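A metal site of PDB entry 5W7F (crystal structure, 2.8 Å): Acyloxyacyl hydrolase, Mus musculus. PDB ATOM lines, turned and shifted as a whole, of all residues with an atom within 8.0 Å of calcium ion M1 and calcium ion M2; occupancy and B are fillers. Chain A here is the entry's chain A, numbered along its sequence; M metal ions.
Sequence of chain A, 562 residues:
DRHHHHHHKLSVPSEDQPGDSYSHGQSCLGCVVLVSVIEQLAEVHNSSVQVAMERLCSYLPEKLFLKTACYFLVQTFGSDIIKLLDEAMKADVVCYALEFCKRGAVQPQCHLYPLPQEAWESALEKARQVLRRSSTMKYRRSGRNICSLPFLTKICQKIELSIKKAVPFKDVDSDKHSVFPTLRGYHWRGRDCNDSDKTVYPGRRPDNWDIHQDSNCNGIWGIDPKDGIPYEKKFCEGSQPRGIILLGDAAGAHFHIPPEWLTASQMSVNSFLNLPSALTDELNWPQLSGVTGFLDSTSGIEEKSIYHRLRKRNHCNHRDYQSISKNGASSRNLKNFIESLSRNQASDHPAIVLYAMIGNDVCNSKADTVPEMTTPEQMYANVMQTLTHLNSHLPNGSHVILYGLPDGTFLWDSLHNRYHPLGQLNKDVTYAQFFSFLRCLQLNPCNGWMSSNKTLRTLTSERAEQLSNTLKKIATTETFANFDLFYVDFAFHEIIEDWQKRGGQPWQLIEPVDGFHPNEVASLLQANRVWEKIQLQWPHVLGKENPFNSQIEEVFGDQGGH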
ATOM      1  N   PRO A 168      20.405 -12.250  11.189  1.00  0.00           N
ATOM      2  CA  PRO A 168      20.229 -11.785   9.813  1.00  0.00           C
ATOM      3  C   PRO A 168      21.424 -12.137   8.951  1.00  0.00           C
ATOM      4  O   PRO A 168      22.584 -11.980   9.342  1.00  0.00           O
ATOM      5  CB  PRO A 168      20.068 -10.267   9.972  1.00  0.00           C
ATOM      6  CG  PRO A 168      20.649  -9.942  11.309  1.00  0.00           C
ATOM      7  CD  PRO A 168      20.404 -11.138  12.163  1.00  0.00           C
ATOM      8  N   LYS A 170      22.101 -10.601   6.089  1.00  0.00           N
ATOM      9  CA  LYS A 170      22.636  -9.320   5.624  1.00  0.00           C
ATOM     10  C   LYS A 170      22.843  -8.441   6.844  1.00  0.00           C
ATOM     11  O   LYS A 170      21.903  -7.791   7.320  1.00  0.00           O
ATOM     12  CB  LYS A 170      21.686  -8.673   4.620  1.00  0.00           C
ATOM     13  CG  LYS A 170      21.446  -9.472   3.353  1.00  0.00           C
ATOM     14  CD  LYS A 170      22.533  -9.250   2.312  1.00  0.00           C
ATOM     15  CE  LYS A 170      22.225  -9.982   1.014  1.00  0.00           C
ATOM     16  NZ  LYS A 170      21.161  -9.322   0.209  1.00  0.00           N
ATOM     17  N   ASP A 171      24.072  -8.404   7.363  1.00  0.00           N
ATOM     18  CA  ASP A 171      24.357  -7.639   8.569  1.00  0.00           C
ATOM     19  C   ASP A 171      25.861  -7.363   8.590  1.00  0.00           C
ATOM     20  O   ASP A 171      26.641  -8.124   9.161  1.00  0.00           O
ATOM     21  CB  ASP A 171      23.912  -8.389   9.818  1.00  0.00           C
ATOM     22  CG  ASP A 171      23.977  -7.535  11.069  1.00  0.00           C
ATOM     23  OD1 ASP A 171      23.973  -8.098  12.178  1.00  0.00           O
ATOM     24  OD2 ASP A 171      24.013  -6.292  10.930  1.00  0.00           O
ATOM     25  N   VAL A 172      26.250  -6.246   7.952  1.00  0.00           N
ATOM     26  CA  VAL A 172      27.670  -5.931   7.810  1.00  0.00           C
ATOM     27  C   VAL A 172      28.289  -5.621   9.169  1.00  0.00           C
ATOM     28  O   VAL A 172      29.393  -6.087   9.490  1.00  0.00           O
ATOM     29  CB  VAL A 172      27.864  -4.769   6.824  1.00  0.00           C
ATOM     30  CG1 VAL A 172      29.350  -4.464   6.640  1.00  0.00           C
ATOM     31  CG2 VAL A 172      27.217  -5.101   5.483  1.00  0.00           C
ATOM     32  N   ASP A 173      27.596  -4.835  10.004  1.00  0.00           N
ATOM     33  CA  ASP A 173      28.145  -4.429  11.295  1.00  0.00           C
ATOM     34  C   ASP A 173      27.964  -5.477  12.379  1.00  0.00           C
ATOM     35  O   ASP A 173      28.507  -5.309  13.472  1.00  0.00           O
ATOM     36  CB  ASP A 173      27.505  -3.112  11.746  1.00  0.00           C
ATOM     37  CG  ASP A 173      25.995  -3.202  11.882  1.00  0.00           C
ATOM     38  OD1 ASP A 173      25.469  -4.328  11.970  1.00  0.00           O
ATOM     39  OD2 ASP A 173      25.336  -2.138  11.907  1.00  0.00           O
ATOM     40  N   SER A 174      27.193  -6.539  12.108  1.00  0.00           N
ATOM     41  CA  SER A 174      27.016  -7.639  13.059  1.00  0.00           C
ATOM     42  C   SER A 174      26.356  -7.183  14.353  1.00  0.00           C
ATOM     43  O   SER A 174      26.672  -7.682  15.433  1.00  0.00           O
ATOM     44  CB  SER A 174      28.356  -8.329  13.355  1.00  0.00           C
ATOM     45  OG  SER A 174      28.829  -9.026  12.211  1.00  0.00           O
ATOM     46  N   ASP A 175      25.438  -6.214  14.262  1.00  0.00           N
ATOM     47  CA  ASP A 175      24.592  -5.846  15.387  1.00  0.00           C
ATOM     48  C   ASP A 175      23.289  -6.629  15.436  1.00  0.00           C
ATOM     49  O   ASP A 175      22.436  -6.344  16.275  1.00  0.00           O
ATOM     50  CB  ASP A 175      24.287  -4.341  15.355  1.00  0.00           C
ATOM     51  CG  ASP A 175      23.542  -3.919  14.104  1.00  0.00           C
ATOM     52  OD1 ASP A 175      23.177  -4.801  13.294  1.00  0.00           O
ATOM     53  OD2 ASP A 175      23.313  -2.707  13.944  1.00  0.00           O
ATOM     54  N   LYS A 176      23.108  -7.607  14.534  1.00  0.00           N
ATOM     55  CA  LYS A 176      21.957  -8.504  14.485  1.00  0.00           C
ATOM     56  C   LYS A 176      20.675  -7.833  14.004  1.00  0.00           C
ATOM     57  O   LYS A 176      19.601  -8.455  14.061  1.00  0.00           O
ATOM     58  CB  LYS A 176      21.700  -9.188  15.833  1.00  0.00           C
ATOM     59  CG  LYS A 176      22.630 -10.336  16.115  1.00  0.00           C
ATOM     60  CD  LYS A 176      22.647 -10.680  17.588  1.00  0.00           C
ATOM     61  CE  LYS A 176      23.670 -11.746  17.901  1.00  0.00           C
ATOM     62  NZ  LYS A 176      24.034 -11.734  19.338  1.00  0.00           N
ATOM     63  N   HIS A 177      20.744  -6.594  13.540  1.00  0.00           N
ATOM     64  CA  HIS A 177      19.633  -5.950  12.868  1.00  0.00           C
ATOM     65  C   HIS A 177      20.043  -5.675  11.423  1.00  0.00           C
ATOM     66  O   HIS A 177      21.208  -5.361  11.151  1.00  0.00           O
ATOM     67  CB  HIS A 177      19.229  -4.641  13.571  1.00  0.00           C
ATOM     68  CG  HIS A 177      18.672  -4.851  14.944  1.00  0.00           C
ATOM     69  ND1 HIS A 177      17.378  -4.533  15.285  1.00  0.00           N
ATOM     70  CD2 HIS A 177      19.250  -5.327  16.073  1.00  0.00           C
ATOM     71  CE1 HIS A 177      17.172  -4.813  16.553  1.00  0.00           C
ATOM     72  NE2 HIS A 177      18.293  -5.302  17.065  1.00  0.00           N
ATOM     73  N   SER A 178      19.085  -5.809  10.511  1.00  0.00           N
ATOM     74  CA  SER A 178      19.381  -5.791   9.084  1.00  0.00           C
ATOM     75  C   SER A 178      18.596  -4.692   8.398  1.00  0.00           C
ATOM     76  O   SER A 178      17.639  -4.136   8.936  1.00  0.00           O
ATOM     77  CB  SER A 178      19.049  -7.136   8.446  1.00  0.00           C
ATOM     78  OG  SER A 178      19.348  -7.142   7.065  1.00  0.00           O
ATOM     79  N   VAL A 179      19.020  -4.377   7.169  1.00  0.00           N
ATOM     80  CA  VAL A 179      18.278  -3.502   6.269  1.00  0.00           C
ATOM     81  C   VAL A 179      17.470  -4.289   5.250  1.00  0.00           C
ATOM     82  O   VAL A 179      16.700  -3.693   4.486  1.00  0.00           O
ATOM     83  CB  VAL A 179      19.240  -2.514   5.570  1.00  0.00           C
ATOM     84  CG1 VAL A 179      20.067  -3.222   4.496  1.00  0.00           C
ATOM     85  CG2 VAL A 179      18.469  -1.321   5.004  1.00  0.00           C
ATOM     86  N   GLY A 190      13.478  -4.809  14.496  1.00  0.00           N
ATOM     87  CA  GLY A 190      13.458  -3.473  13.933  1.00  0.00           C
ATOM     88  C   GLY A 190      14.532  -3.296  12.883  1.00  0.00           C
ATOM     89  O   GLY A 190      15.663  -3.783  13.060  1.00  0.00           O
ATOM     90  N   ARG A 191      14.214  -2.607  11.786  1.00  0.00           N
ATOM     91  CA  ARG A 191      15.191  -2.392  10.736  1.00  0.00           C
ATOM     92  C   ARG A 191      16.331  -1.518  11.233  1.00  0.00           C
ATOM     93  O   ARG A 191      16.155  -0.648  12.091  1.00  0.00           O
ATOM     94  CB  ARG A 191      14.541  -1.746   9.511  1.00  0.00           C
ATOM     95  CG  ARG A 191      15.396  -1.815   8.243  1.00  0.00           C
ATOM     96  CD  ARG A 191      15.003  -0.766   7.218  1.00  0.00           C
ATOM     97  NE  ARG A 191      13.587  -0.848   6.840  1.00  0.00           N
ATOM     98  CZ  ARG A 191      13.127  -1.147   5.626  1.00  0.00           C
ATOM     99  NH1 ARG A 191      13.959  -1.406   4.619  1.00  0.00           N
ATOM    100  NH2 ARG A 191      11.819  -1.177   5.405  1.00  0.00           N
ATOM    101  N   ASP A 192      17.518  -1.763  10.683  1.00  0.00           N
ATOM    102  CA  ASP A 192      18.711  -1.007  11.047  1.00  0.00           C
ATOM    103  C   ASP A 192      18.859   0.183  10.113  1.00  0.00           C
ATOM    104  O   ASP A 192      18.858   0.016   8.886  1.00  0.00           O
ATOM    105  CB  ASP A 192      19.954  -1.902  10.988  1.00  0.00           C
ATOM    106  CG  ASP A 192      21.161  -1.264  11.649  1.00  0.00           C
ATOM    107  OD1 ASP A 192      21.001  -0.226  12.327  1.00  0.00           O
ATOM    108  OD2 ASP A 192      22.282  -1.798  11.488  1.00  0.00           O
ATOM    109  N   CYS A 193      18.969   1.373  10.693  1.00  0.00           N
ATOM    110  CA  CYS A 193      19.110   2.587   9.896  1.00  0.00           C
ATOM    111  C   CYS A 193      20.550   2.835   9.488  1.00  0.00           C
ATOM    112  O   CYS A 193      20.807   3.344   8.389  1.00  0.00           O
ATOM    113  CB  CYS A 193      18.558   3.792  10.660  1.00  0.00           C
ATOM    114  SG  CYS A 193      19.224   3.995  12.338  1.00  0.00           S
ATOM    115  N   ASN A 194      21.512   2.476  10.343  1.00  0.00           N
ATOM    116  CA  ASN A 194      22.936   2.588  10.041  1.00  0.00           C
ATOM    117  C   ASN A 194      23.539   1.190  10.107  1.00  0.00           C
ATOM    118  O   ASN A 194      23.965   0.732  11.167  1.00  0.00           O
ATOM    119  CB  ASN A 194      23.629   3.550  11.018  1.00  0.00           C
ATOM    120  CG  ASN A 194      24.861   4.204  10.423  1.00  0.00           C
ATOM    121  OD1 ASN A 194      25.478   3.682   9.490  1.00  0.00           O
ATOM    122  ND2 ASN A 194      25.236   5.361  10.965  1.00  0.00           N
ATOM    123  N   ASP A 195      23.552   0.499   8.962  1.00  0.00           N
ATOM    124  CA  ASP A 195      24.116  -0.848   8.907  1.00  0.00           C
ATOM    125  C   ASP A 195      25.630  -0.840   9.028  1.00  0.00           C
ATOM    126  O   ASP A 195      26.219  -1.888   9.306  1.00  0.00           O
ATOM    127  CB  ASP A 195      23.697  -1.542   7.612  1.00  0.00           C
ATOM    128  CG  ASP A 195      23.891  -3.045   7.667  1.00  0.00           C
ATOM    129  OD1 ASP A 195      23.752  -3.629   8.757  1.00  0.00           O
ATOM    130  OD2 ASP A 195      24.186  -3.641   6.609  1.00  0.00           O
ATOM    131  N   SER A 196      26.283   0.304   8.802  1.00  0.00           N
ATOM    132  CA  SER A 196      27.730   0.396   8.940  1.00  0.00           C
ATOM    133  C   SER A 196      28.154   0.527  10.396  1.00  0.00           C
ATOM    134  O   SER A 196      29.261   0.102  10.752  1.00  0.00           O
ATOM    135  CB  SER A 196      28.262   1.580   8.136  1.00  0.00           C
ATOM    136  OG  SER A 196      28.028   1.397   6.749  1.00  0.00           O
ATOM    137  N   ASP A 197      27.308   1.103  11.244  1.00  0.00           N
ATOM    138  CA  ASP A 197      27.630   1.356  12.635  1.00  0.00           C
ATOM    139  C   ASP A 197      27.088   0.207  13.491  1.00  0.00           C
ATOM    140  O   ASP A 197      25.874  -0.038  13.510  1.00  0.00           O
ATOM    141  CB  ASP A 197      27.043   2.695  13.087  1.00  0.00           C
ATOM    142  CG  ASP A 197      27.702   3.232  14.333  1.00  0.00           C
ATOM    143  OD1 ASP A 197      28.089   2.427  15.213  1.00  0.00           O
ATOM    144  OD2 ASP A 197      27.838   4.467  14.451  1.00  0.00           O
ATOM    145  N   LYS A 198      27.983  -0.487  14.200  1.00  0.00           N
ATOM    146  CA  LYS A 198      27.556  -1.558  15.095  1.00  0.00           C
ATOM    147  C   LYS A 198      27.077  -1.041  16.446  1.00  0.00           C
ATOM    148  O   LYS A 198      26.714  -1.851  17.310  1.00  0.00           O
ATOM    149  CB  LYS A 198      28.695  -2.562  15.307  1.00  0.00           C
ATOM    150  CG  LYS A 198      29.879  -2.019  16.089  1.00  0.00           C
ATOM    151  CD  LYS A 198      30.945  -3.094  16.250  1.00  0.00           C
ATOM    152  CE  LYS A 198      32.211  -2.544  16.898  1.00  0.00           C
ATOM    153  NZ  LYS A 198      33.256  -3.598  17.052  1.00  0.00           N
ATOM    154  N   THR A 199      27.055   0.270  16.649  1.00  0.00           N
ATOM    155  CA  THR A 199      26.486   0.879  17.846  1.00  0.00           C
ATOM    156  C   THR A 199      25.086   1.430  17.599  1.00  0.00           C
ATOM    157  O   THR A 199      24.485   1.979  18.525  1.00  0.00           O
ATOM    158  CB  THR A 199      27.393   2.007  18.364  1.00  0.00           C
ATOM    159  OG1 THR A 199      27.236   3.173  17.539  1.00  0.00           O
ATOM    160  CG2 THR A 199      28.852   1.574  18.368  1.00  0.00           C
ATOM    161  N   VAL A 200      24.573   1.305  16.375  1.00  0.00           N
ATOM    162  CA  VAL A 200      23.254   1.824  16.014  1.00  0.00           C
ATOM    163  C   VAL A 200      22.323   0.630  15.842  1.00  0.00           C
ATOM    164  O   VAL A 200      22.490  -0.183  14.923  1.00  0.00           O
ATOM    165  CB  VAL A 200      23.309   2.662  14.731  1.00  0.00           C
ATOM    166  CG1 VAL A 200      21.924   3.116  14.313  1.00  0.00           C
ATOM    167  CG2 VAL A 200      24.238   3.864  14.932  1.00  0.00           C
ATOM    168  N   TYR A 201      21.335   0.522  16.726  1.00  0.00           N
ATOM    169  CA  TYR A 201      20.345  -0.546  16.640  1.00  0.00           C
ATOM    170  C   TYR A 201      19.139  -0.154  17.484  1.00  0.00           C
ATOM    171  O   TYR A 201      19.302   0.547  18.496  1.00  0.00           O
ATOM    172  CB  TYR A 201      20.931  -1.880  17.133  1.00  0.00           C
ATOM    173  CG  TYR A 201      21.543  -1.824  18.508  1.00  0.00           C
ATOM    174  CD1 TYR A 201      20.745  -1.787  19.644  1.00  0.00           C
ATOM    175  CD2 TYR A 201      22.918  -1.832  18.678  1.00  0.00           C
ATOM    176  CE1 TYR A 201      21.298  -1.737  20.910  1.00  0.00           C
ATOM    177  CE2 TYR A 201      23.485  -1.784  19.941  1.00  0.00           C
ATOM    178  CZ  TYR A 201      22.663  -1.735  21.053  1.00  0.00           C
ATOM    179  OH  TYR A 201      23.223  -1.679  22.314  1.00  0.00           O
ATOM    180  N   PRO A 202      17.928  -0.565  17.107  1.00  0.00           N
ATOM    181  CA  PRO A 202      16.759  -0.246  17.924  1.00  0.00           C
ATOM    182  C   PRO A 202      16.910  -0.744  19.357  1.00  0.00           C
ATOM    183  O   PRO A 202      17.542  -1.772  19.616  1.00  0.00           O
ATOM    184  CB  PRO A 202      15.606  -0.965  17.202  1.00  0.00           C
ATOM    185  CG  PRO A 202      16.074  -1.078  15.784  1.00  0.00           C
ATOM    186  CD  PRO A 202      17.560  -1.241  15.850  1.00  0.00           C
ATOM    187  N   ASP A 214      20.576   9.358  14.370  1.00  0.00           N
ATOM    188  CA  ASP A 214      19.671   8.517  15.142  1.00  0.00           C
ATOM    189  C   ASP A 214      20.419   7.291  15.673  1.00  0.00           C
ATOM    190  O   ASP A 214      20.945   6.492  14.889  1.00  0.00           O
ATOM    191  CB  ASP A 214      18.490   8.091  14.277  1.00  0.00           C
ATOM    192  CG  ASP A 214      17.255   7.744  15.094  1.00  0.00           C
ATOM    193  OD1 ASP A 214      16.152   7.738  14.522  1.00  0.00           O
ATOM    194  OD2 ASP A 214      17.391   7.499  16.309  1.00  0.00           O
ATOM    195  N   SER A 215      20.468   7.156  16.998  1.00  0.00           N
ATOM    196  CA  SER A 215      21.247   6.084  17.615  1.00  0.00           C
ATOM    197  C   SER A 215      20.464   4.775  17.666  1.00  0.00           C
ATOM    198  O   SER A 215      21.059   3.703  17.499  1.00  0.00           O
ATOM    199  CB  SER A 215      21.670   6.496  19.030  1.00  0.00           C
ATOM    200  OG  SER A 215      20.537   6.752  19.849  1.00  0.00           O
ATOM    201  N   CYS A 217      17.565   4.109  15.755  1.00  0.00           N
ATOM    202  CA  CYS A 217      16.724   3.966  14.561  1.00  0.00           C
ATOM    203  C   CYS A 217      15.239   4.121  14.864  1.00  0.00           C
ATOM    204  O   CYS A 217      14.398   3.639  14.107  1.00  0.00           O
ATOM    205  CB  CYS A 217      16.975   2.617  13.875  1.00  0.00           C
ATOM    206  SG  CYS A 217      18.674   2.318  13.329  1.00  0.00           S
HETATM  207 CA    CA M   1      23.171  -3.929  11.150  1.00  0.00          CA
HETATM  208 CA    CA M   2      23.653  -0.666  13.038  1.00  0.00          CA
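The side-chain sulfur (SG) of Cys 193 forms a disulfide with the side-chain sulfur (SG) of Cys 217 (2.0 Å).
A ring nitrogen (ND1) of His 177 sits at hydrogen-bond distance from the backbone carbonyl oxygen (O) of Gly 190 (2.9 Å).
The side-chain hydroxyl of Thr 199 is in hydrogen-bond range of the side-chain carboxylate of Asp 197 (2.6 Å).
The side-chain carboxylate (OD1) of Asp 171 sits at hydrogen-bond distance from the backbone NH (N) of Lys 176 (2.6 Å).
The side-chain carboxylate (OD2) of Asp 171 sits close to the backbone NH (N) of Ser 174 (3.4 Å).
The backbone NH (N) of Asp 192 is in hydrogen-bond range of the backbone carbonyl oxygen (O) of Ser 178, at 2.9 Å.
The nearest printed residue that does not touch calcium ion M2 is Asp 195 (4.2 Å).
Calcium ion M1 is bound by the side-chain carboxylate (OD1) of Asp 175 (2.3 Å), the side-chain carboxylate (OD2) of Asp 192 (2.3 Å), the backbone carbonyl oxygen (O) of His 177 (2.4 Å), the side-chain carboxylate (OD1) of Asp 173 (2.5 Å), the side-chain carboxylate (OD1) of Asp 195 (2.5 Å) and the side-chain carboxylate (OD2) of Asp 171 (2.5 Å).
Calcium ion M1 has six donor atoms within binding distance.
Slightly farther from calcium ion M1 lies OD2 of Asp 173 (2.9 Å).
Slightly farther from calcium ion M1 lies OD2 of Asp 175 (3.1 Å).
Calcium ion M2 is bound by the side-chain carboxylate (OD2) of Asp 175 (2.3 Å), the backbone carbonyl oxygen (O) of Val 200 (2.3 Å), the backbone carbonyl oxygen (O) of Asp 197 (2.4 Å), the backbone carbonyl oxygen (O) of Asn 194 (2.4 Å), the side-chain carboxylate (OD2) of Asp 192 (2.4 Å), the side-chain carboxylate (OD2) of Asp 173 (2.5 Å) and the side-chain carboxylate (OD1) of Asp 192 (2.8 Å).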
